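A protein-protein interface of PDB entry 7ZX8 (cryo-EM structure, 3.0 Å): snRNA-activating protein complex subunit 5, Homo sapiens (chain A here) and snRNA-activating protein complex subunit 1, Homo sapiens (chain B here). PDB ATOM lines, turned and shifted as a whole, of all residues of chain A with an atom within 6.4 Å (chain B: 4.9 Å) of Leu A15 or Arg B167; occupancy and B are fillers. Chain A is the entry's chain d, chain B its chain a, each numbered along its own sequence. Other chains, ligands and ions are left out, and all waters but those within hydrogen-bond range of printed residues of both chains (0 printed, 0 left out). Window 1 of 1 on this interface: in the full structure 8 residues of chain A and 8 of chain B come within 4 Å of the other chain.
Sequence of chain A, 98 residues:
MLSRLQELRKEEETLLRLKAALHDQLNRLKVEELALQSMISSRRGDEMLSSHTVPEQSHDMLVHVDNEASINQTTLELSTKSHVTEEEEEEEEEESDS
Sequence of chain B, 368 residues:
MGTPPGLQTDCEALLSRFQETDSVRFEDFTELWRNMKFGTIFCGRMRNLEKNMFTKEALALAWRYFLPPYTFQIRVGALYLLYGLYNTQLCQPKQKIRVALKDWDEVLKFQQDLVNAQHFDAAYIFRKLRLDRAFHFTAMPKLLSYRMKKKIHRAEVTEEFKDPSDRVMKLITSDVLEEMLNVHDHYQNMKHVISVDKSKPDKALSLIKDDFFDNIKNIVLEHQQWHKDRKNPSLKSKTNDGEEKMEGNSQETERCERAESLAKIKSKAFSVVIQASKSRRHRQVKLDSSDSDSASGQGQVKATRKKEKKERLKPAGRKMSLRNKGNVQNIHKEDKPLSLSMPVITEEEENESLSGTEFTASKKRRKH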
ATOM      1  N   ARG A   4     -11.807  -4.001  10.157  1.00  0.00           N
ATOM      2  CA  ARG A   4     -10.450  -4.330   9.739  1.00  0.00           C
ATOM      3  C   ARG A   4      -9.746  -5.163  10.800  1.00  0.00           C
ATOM      4  O   ARG A   4      -8.961  -6.060  10.475  1.00  0.00           O
ATOM      5  CB  ARG A   4      -9.666  -3.050   9.448  1.00  0.00           C
ATOM      6  CG  ARG A   4      -8.359  -3.273   8.699  1.00  0.00           C
ATOM      7  CD  ARG A   4      -8.595  -3.827   7.301  1.00  0.00           C
ATOM      8  NE  ARG A   4      -8.147  -5.211   7.177  1.00  0.00           N
ATOM      9  CZ  ARG A   4      -8.204  -5.919   6.052  1.00  0.00           C
ATOM     10  NH1 ARG A   4      -8.694  -5.378   4.944  1.00  0.00           N
ATOM     11  NH2 ARG A   4      -7.773  -7.173   6.037  1.00  0.00           N
ATOM     12  N   LEU A   8      -8.189  -8.789  10.006  1.00  0.00           N
ATOM     13  CA  LEU A   8      -6.780  -9.058  10.269  1.00  0.00           C
ATOM     14  C   LEU A   8      -6.612 -10.232  11.224  1.00  0.00           C
ATOM     15  O   LEU A   8      -5.736 -11.079  11.025  1.00  0.00           O
ATOM     16  CB  LEU A   8      -6.106  -7.807  10.833  1.00  0.00           C
ATOM     17  CG  LEU A   8      -6.024  -6.608   9.887  1.00  0.00           C
ATOM     18  CD1 LEU A   8      -5.814  -5.321  10.670  1.00  0.00           C
ATOM     19  CD2 LEU A   8      -4.913  -6.803   8.867  1.00  0.00           C
ATOM     20  N   LYS A  10      -8.705 -12.762  11.774  1.00  0.00           N
ATOM     21  CA  LYS A  10      -9.045 -14.019  11.117  1.00  0.00           C
ATOM     22  C   LYS A  10      -7.954 -14.439  10.143  1.00  0.00           C
ATOM     23  O   LYS A  10      -7.648 -15.630  10.027  1.00  0.00           O
ATOM     24  CB  LYS A  10     -10.387 -13.915  10.398  1.00  0.00           C
ATOM     25  CG  LYS A  10     -10.803 -15.219   9.721  1.00  0.00           C
ATOM     26  CD  LYS A  10     -10.916 -16.366  10.714  1.00  0.00           C
ATOM     27  CE  LYS A  10     -11.429 -17.631  10.051  1.00  0.00           C
ATOM     28  NZ  LYS A  10     -11.555 -18.745  11.029  1.00  0.00           N
ATOM     29  N   GLU A  11      -7.361 -13.483   9.421  1.00  0.00           N
ATOM     30  CA  GLU A  11      -6.207 -13.824   8.596  1.00  0.00           C
ATOM     31  C   GLU A  11      -5.060 -14.348   9.450  1.00  0.00           C
ATOM     32  O   GLU A  11      -4.342 -15.270   9.040  1.00  0.00           O
ATOM     33  CB  GLU A  11      -5.757 -12.606   7.789  1.00  0.00           C
ATOM     34  CG  GLU A  11      -6.735 -12.191   6.702  1.00  0.00           C
ATOM     35  CD  GLU A  11      -6.278 -10.960   5.946  1.00  0.00           C
ATOM     36  OE1 GLU A  11      -5.262 -10.356   6.346  1.00  0.00           O
ATOM     37  OE2 GLU A  11      -6.937 -10.595   4.950  1.00  0.00           O
ATOM     38  N   GLU A  12      -4.879 -13.772  10.640  1.00  0.00           N
ATOM     39  CA  GLU A  12      -3.847 -14.238  11.558  1.00  0.00           C
ATOM     40  C   GLU A  12      -4.088 -15.689  11.956  1.00  0.00           C
ATOM     41  O   GLU A  12      -3.165 -16.508  11.946  1.00  0.00           O
ATOM     42  CB  GLU A  12      -3.813 -13.327  12.787  1.00  0.00           C
ATOM     43  CG  GLU A  12      -2.672 -13.593  13.751  1.00  0.00           C
ATOM     44  CD  GLU A  12      -2.893 -12.950  15.106  1.00  0.00           C
ATOM     45  OE1 GLU A  12      -3.325 -13.660  16.040  1.00  0.00           O
ATOM     46  OE2 GLU A  12      -2.633 -11.735  15.239  1.00  0.00           O
ATOM     47  N   GLU A  13      -5.331 -16.026  12.308  1.00  0.00           N
ATOM     48  CA  GLU A  13      -5.644 -17.414  12.651  1.00  0.00           C
ATOM     49  C   GLU A  13      -5.470 -18.334  11.448  1.00  0.00           C
ATOM     50  O   GLU A  13      -4.981 -19.462  11.587  1.00  0.00           O
ATOM     51  CB  GLU A  13      -7.068 -17.528  13.202  1.00  0.00           C
ATOM     52  CG  GLU A  13      -7.437 -16.512  14.273  1.00  0.00           C
ATOM     53  CD  GLU A  13      -6.345 -16.312  15.308  1.00  0.00           C
ATOM     54  OE1 GLU A  13      -6.252 -15.198  15.864  1.00  0.00           O
ATOM     55  OE2 GLU A  13      -5.589 -17.269  15.577  1.00  0.00           O
ATOM     56  N   THR A  14      -5.878 -17.877  10.263  1.00  0.00           N
ATOM     57  CA  THR A  14      -5.690 -18.661   9.047  1.00  0.00           C
ATOM     58  C   THR A  14      -4.225 -19.025   8.859  1.00  0.00           C
ATOM     59  O   THR A  14      -3.873 -20.199   8.670  1.00  0.00           O
ATOM     60  CB  THR A  14      -6.194 -17.865   7.840  1.00  0.00           C
ATOM     61  OG1 THR A  14      -7.622 -17.762   7.882  1.00  0.00           O
ATOM     62  CG2 THR A  14      -5.757 -18.521   6.533  1.00  0.00           C
ATOM     63  N   LEU A  15      -3.355 -18.020   8.912  1.00  0.00           N
ATOM     64  CA  LEU A  15      -1.937 -18.257   8.683  1.00  0.00           C
ATOM     65  C   LEU A  15      -1.293 -19.021   9.836  1.00  0.00           C
ATOM     66  O   LEU A  15      -0.364 -19.799   9.606  1.00  0.00           O
ATOM     67  CB  LEU A  15      -1.247 -16.919   8.388  1.00  0.00           C
ATOM     68  CG  LEU A  15      -1.257 -15.798   9.431  1.00  0.00           C
ATOM     69  CD1 LEU A  15      -0.174 -15.942  10.473  1.00  0.00           C
ATOM     70  CD2 LEU A  15      -1.148 -14.442   8.736  1.00  0.00           C
ATOM     71  N   LEU A  16      -1.792 -18.866  11.067  1.00  0.00           N
ATOM     72  CA  LEU A  16      -1.327 -19.724  12.157  1.00  0.00           C
ATOM     73  C   LEU A  16      -1.667 -21.186  11.904  1.00  0.00           C
ATOM     74  O   LEU A  16      -0.841 -22.070  12.150  1.00  0.00           O
ATOM     75  CB  LEU A  16      -1.916 -19.273  13.496  1.00  0.00           C
ATOM     76  CG  LEU A  16      -1.135 -18.254  14.333  1.00  0.00           C
ATOM     77  CD1 LEU A  16       0.194 -18.847  14.776  1.00  0.00           C
ATOM     78  CD2 LEU A  16      -0.901 -16.967  13.586  1.00  0.00           C
ATOM     79  N   ARG A  17      -2.883 -21.467  11.435  1.00  0.00           N
ATOM     80  CA  ARG A  17      -3.251 -22.854  11.157  1.00  0.00           C
ATOM     81  C   ARG A  17      -2.424 -23.422  10.011  1.00  0.00           C
ATOM     82  O   ARG A  17      -1.974 -24.575  10.068  1.00  0.00           O
ATOM     83  CB  ARG A  17      -4.744 -22.947  10.850  1.00  0.00           C
ATOM     84  CG  ARG A  17      -5.618 -22.941  12.091  1.00  0.00           C
ATOM     85  CD  ARG A  17      -7.077 -22.696  11.752  1.00  0.00           C
ATOM     86  NE  ARG A  17      -7.348 -21.279  11.530  1.00  0.00           N
ATOM     87  CZ  ARG A  17      -8.440 -20.806  10.939  1.00  0.00           C
ATOM     88  NH1 ARG A  17      -9.381 -21.636  10.504  1.00  0.00           N
ATOM     89  NH2 ARG A  17      -8.593 -19.499  10.780  1.00  0.00           N
ATOM     90  N   LEU A  18      -2.209 -22.623   8.962  1.00  0.00           N
ATOM     91  CA  LEU A  18      -1.356 -23.074   7.867  1.00  0.00           C
ATOM     92  C   LEU A  18       0.060 -23.353   8.359  1.00  0.00           C
ATOM     93  O   LEU A  18       0.667 -24.366   7.987  1.00  0.00           O
ATOM     94  CB  LEU A  18      -1.346 -22.034   6.746  1.00  0.00           C
ATOM     95  CG  LEU A  18      -2.697 -21.739   6.087  1.00  0.00           C
ATOM     96  CD1 LEU A  18      -2.562 -20.622   5.062  1.00  0.00           C
ATOM     97  CD2 LEU A  18      -3.271 -22.991   5.437  1.00  0.00           C
ATOM     98  N   LYS A  19       0.600 -22.473   9.207  1.00  0.00           N
ATOM     99  CA  LYS A  19       1.935 -22.689   9.752  1.00  0.00           C
ATOM    100  C   LYS A  19       1.986 -23.933  10.628  1.00  0.00           C
ATOM    101  O   LYS A  19       2.971 -24.671  10.599  1.00  0.00           O
ATOM    102  CB  LYS A  19       2.389 -21.463  10.543  1.00  0.00           C
ATOM    103  CG  LYS A  19       2.681 -20.240   9.698  1.00  0.00           C
ATOM    104  CD  LYS A  19       3.119 -19.081  10.574  1.00  0.00           C
ATOM    105  CE  LYS A  19       3.540 -17.885   9.747  1.00  0.00           C
ATOM    106  NZ  LYS A  19       2.395 -17.299   9.001  1.00  0.00           N
ATOM    107  N   ALA A  20       0.945 -24.179  11.425  1.00  0.00           N
ATOM    108  CA  ALA A  20       0.928 -25.378  12.257  1.00  0.00           C
ATOM    109  C   ALA A  20       0.943 -26.634  11.397  1.00  0.00           C
ATOM    110  O   ALA A  20       1.715 -27.571  11.648  1.00  0.00           O
ATOM    111  CB  ALA A  20      -0.300 -25.367  13.169  1.00  0.00           C
ATOM    112  N   SER B 165      -8.738  -7.524   0.531  1.00  0.00           N
ATOM    113  CA  SER B 165      -7.838  -8.461  -0.126  1.00  0.00           C
ATOM    114  C   SER B 165      -7.592  -9.639   0.810  1.00  0.00           C
ATOM    115  O   SER B 165      -6.902  -9.499   1.823  1.00  0.00           O
ATOM    116  CB  SER B 165      -6.514  -7.788  -0.493  1.00  0.00           C
ATOM    117  OG  SER B 165      -5.624  -8.711  -1.092  1.00  0.00           O
ATOM    118  N   ASP B 166      -8.229 -10.783   0.542  1.00  0.00           N
ATOM    119  CA  ASP B 166      -8.153 -11.927   1.495  1.00  0.00           C
ATOM    120  C   ASP B 166      -6.752 -12.546   1.547  1.00  0.00           C
ATOM    121  O   ASP B 166      -6.205 -12.848   0.483  1.00  0.00           O
ATOM    122  CB  ASP B 166      -9.209 -12.988   1.176  1.00  0.00           C
ATOM    123  CG  ASP B 166     -10.016 -13.414   2.391  1.00  0.00           C
ATOM    124  OD1 ASP B 166      -9.527 -13.204   3.519  1.00  0.00           O
ATOM    125  OD2 ASP B 166     -11.124 -13.949   2.197  1.00  0.00           O
ATOM    126  N   ARG B 167      -6.190 -12.723   2.746  1.00  0.00           N
ATOM    127  CA  ARG B 167      -4.884 -13.429   2.868  1.00  0.00           C
ATOM    128  C   ARG B 167      -5.059 -14.891   2.441  1.00  0.00           C
ATOM    129  O   ARG B 167      -4.102 -15.457   1.904  1.00  0.00           O
ATOM    130  CB  ARG B 167      -4.296 -13.317   4.277  1.00  0.00           C
ATOM    131  CG  ARG B 167      -2.798 -13.053   4.292  1.00  0.00           C
ATOM    132  CD  ARG B 167      -2.251 -12.792   5.682  1.00  0.00           C
ATOM    133  NE  ARG B 167      -2.696 -11.518   6.229  1.00  0.00           N
ATOM    134  CZ  ARG B 167      -1.932 -10.693   6.934  1.00  0.00           C
ATOM    135  NH1 ARG B 167      -2.431  -9.556   7.389  1.00  0.00           N
ATOM    136  NH2 ARG B 167      -0.672 -11.004   7.180  1.00  0.00           N
ATOM    137  N   VAL B 168      -6.211 -15.494   2.750  1.00  0.00           N
ATOM    138  CA  VAL B 168      -6.468 -16.927   2.411  1.00  0.00           C
ATOM    139  C   VAL B 168      -6.050 -17.218   0.963  1.00  0.00           C
ATOM    140  O   VAL B 168      -5.255 -18.141   0.776  1.00  0.00           O
ATOM    141  CB  VAL B 168      -7.937 -17.300   2.677  1.00  0.00           C
ATOM    142  CG1 VAL B 168      -8.122 -18.804   2.807  1.00  0.00           C
ATOM    143  CG2 VAL B 168      -8.463 -16.594   3.917  1.00  0.00           C
ATOM    144  N   MET B 169      -6.574 -16.477  -0.018  1.00  0.00           N
ATOM    145  CA  MET B 169      -6.222 -16.670  -1.418  1.00  0.00           C
ATOM    146  C   MET B 169      -4.750 -16.398  -1.686  1.00  0.00           C
ATOM    147  O   MET B 169      -4.181 -16.993  -2.606  1.00  0.00           O
ATOM    148  CB  MET B 169      -7.087 -15.787  -2.317  1.00  0.00           C
ATOM    149  CG  MET B 169      -7.105 -14.321  -1.933  1.00  0.00           C
ATOM    150  SD  MET B 169      -8.380 -13.388  -2.802  1.00  0.00           S
ATOM    151  CE  MET B 169      -7.735 -11.726  -2.671  1.00  0.00           C
ATOM    152  N   LYS B 170      -4.117 -15.512  -0.909  1.00  0.00           N
ATOM    153  CA  LYS B 170      -2.669 -15.371  -0.998  1.00  0.00           C
ATOM    154  C   LYS B 170      -1.964 -16.619  -0.487  1.00  0.00           C
ATOM    155  O   LYS B 170      -0.868 -16.948  -0.957  1.00  0.00           O
ATOM    156  CB  LYS B 170      -2.195 -14.146  -0.213  1.00  0.00           C
ATOM    157  CG  LYS B 170      -3.020 -12.889  -0.439  1.00  0.00           C
ATOM    158  CD  LYS B 170      -3.098 -12.524  -1.914  1.00  0.00           C
ATOM    159  CE  LYS B 170      -3.921 -11.260  -2.118  1.00  0.00           C
ATOM    160  NZ  LYS B 170      -4.900 -11.051  -1.016  1.00  0.00           N
ATOM    161  N   LEU B 171      -2.572 -17.316   0.468  1.00  0.00           N
ATOM    162  CA  LEU B 171      -1.971 -18.538   0.993  1.00  0.00           C
ATOM    163  C   LEU B 171      -2.325 -19.743   0.134  1.00  0.00           C
ATOM    164  O   LEU B 171      -1.442 -20.494  -0.291  1.00  0.00           O
ATOM    165  CB  LEU B 171      -2.408 -18.762   2.438  1.00  0.00           C
ATOM    166  CG  LEU B 171      -1.953 -17.685   3.424  1.00  0.00           C
ATOM    167  CD1 LEU B 171      -2.904 -17.592   4.604  1.00  0.00           C
ATOM    168  CD2 LEU B 171      -0.532 -17.958   3.891  1.00  0.00           C
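The side-chain carboxylate (OE1) of Glu A11 is in salt-bridge range of the guanidinium group (NE) of Arg B167, at 2.8 Å.
OE2 of Glu A11 sits close to O of Ser B165, at 3.3 Å.
The side-chain hydroxyl (OG) of Ser B165 is in hydrogen-bond range of the side-chain amino group (NZ) of Lys B170 (2.5 Å).
O of Asp B166 lies within hydrogen-bond range of NZ of Lys B170 (2.7 Å).
The side-chain carboxylate of Glu A11 lies within salt-bridge range of the guanidinium group of Arg A4 (3.7 Å).
The backbone carbonyl oxygen (O) of Lys A10 lies within hydrogen-bond range of the side-chain hydroxyl (OG1) of Thr A14 (3.0 Å).
Among the printed residues, merely in contact across the chains: Leu A18 with Leu B171 (3.1 Å), Thr A14 with Leu B171 (3.6 Å), Leu A15 with Arg B167 (3.6 Å), Glu A11 with Asp B166 (3.9 Å) and Leu A8 with Arg B167 (3.99 Å).
Of chain B, only Arg B167 (3.6 Å) comes within 4 Å of Leu A15.
Printed residues of chain A within 4 Å of Arg B167: Leu A8 (3.99 Å), Glu A11 (2.8 Å) and Leu A15 (3.6 Å).
Of the printed residues of chain B, Glu A11 touches Ser B165, Asp B166 and Arg B167.
Of the printed residues of chain A, Asp B166 touches Glu A11.
Lys A19 touches none of the printed residues of chain B.
Val B168 touches none of the printed residues of chain A.
Of the 7 printed residues of chain B, 4 touch a printed residue of chain A.
Hydrophobic or aromatic side chains of chain B within 4 Å of the printed part of chain A: Leu B171.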
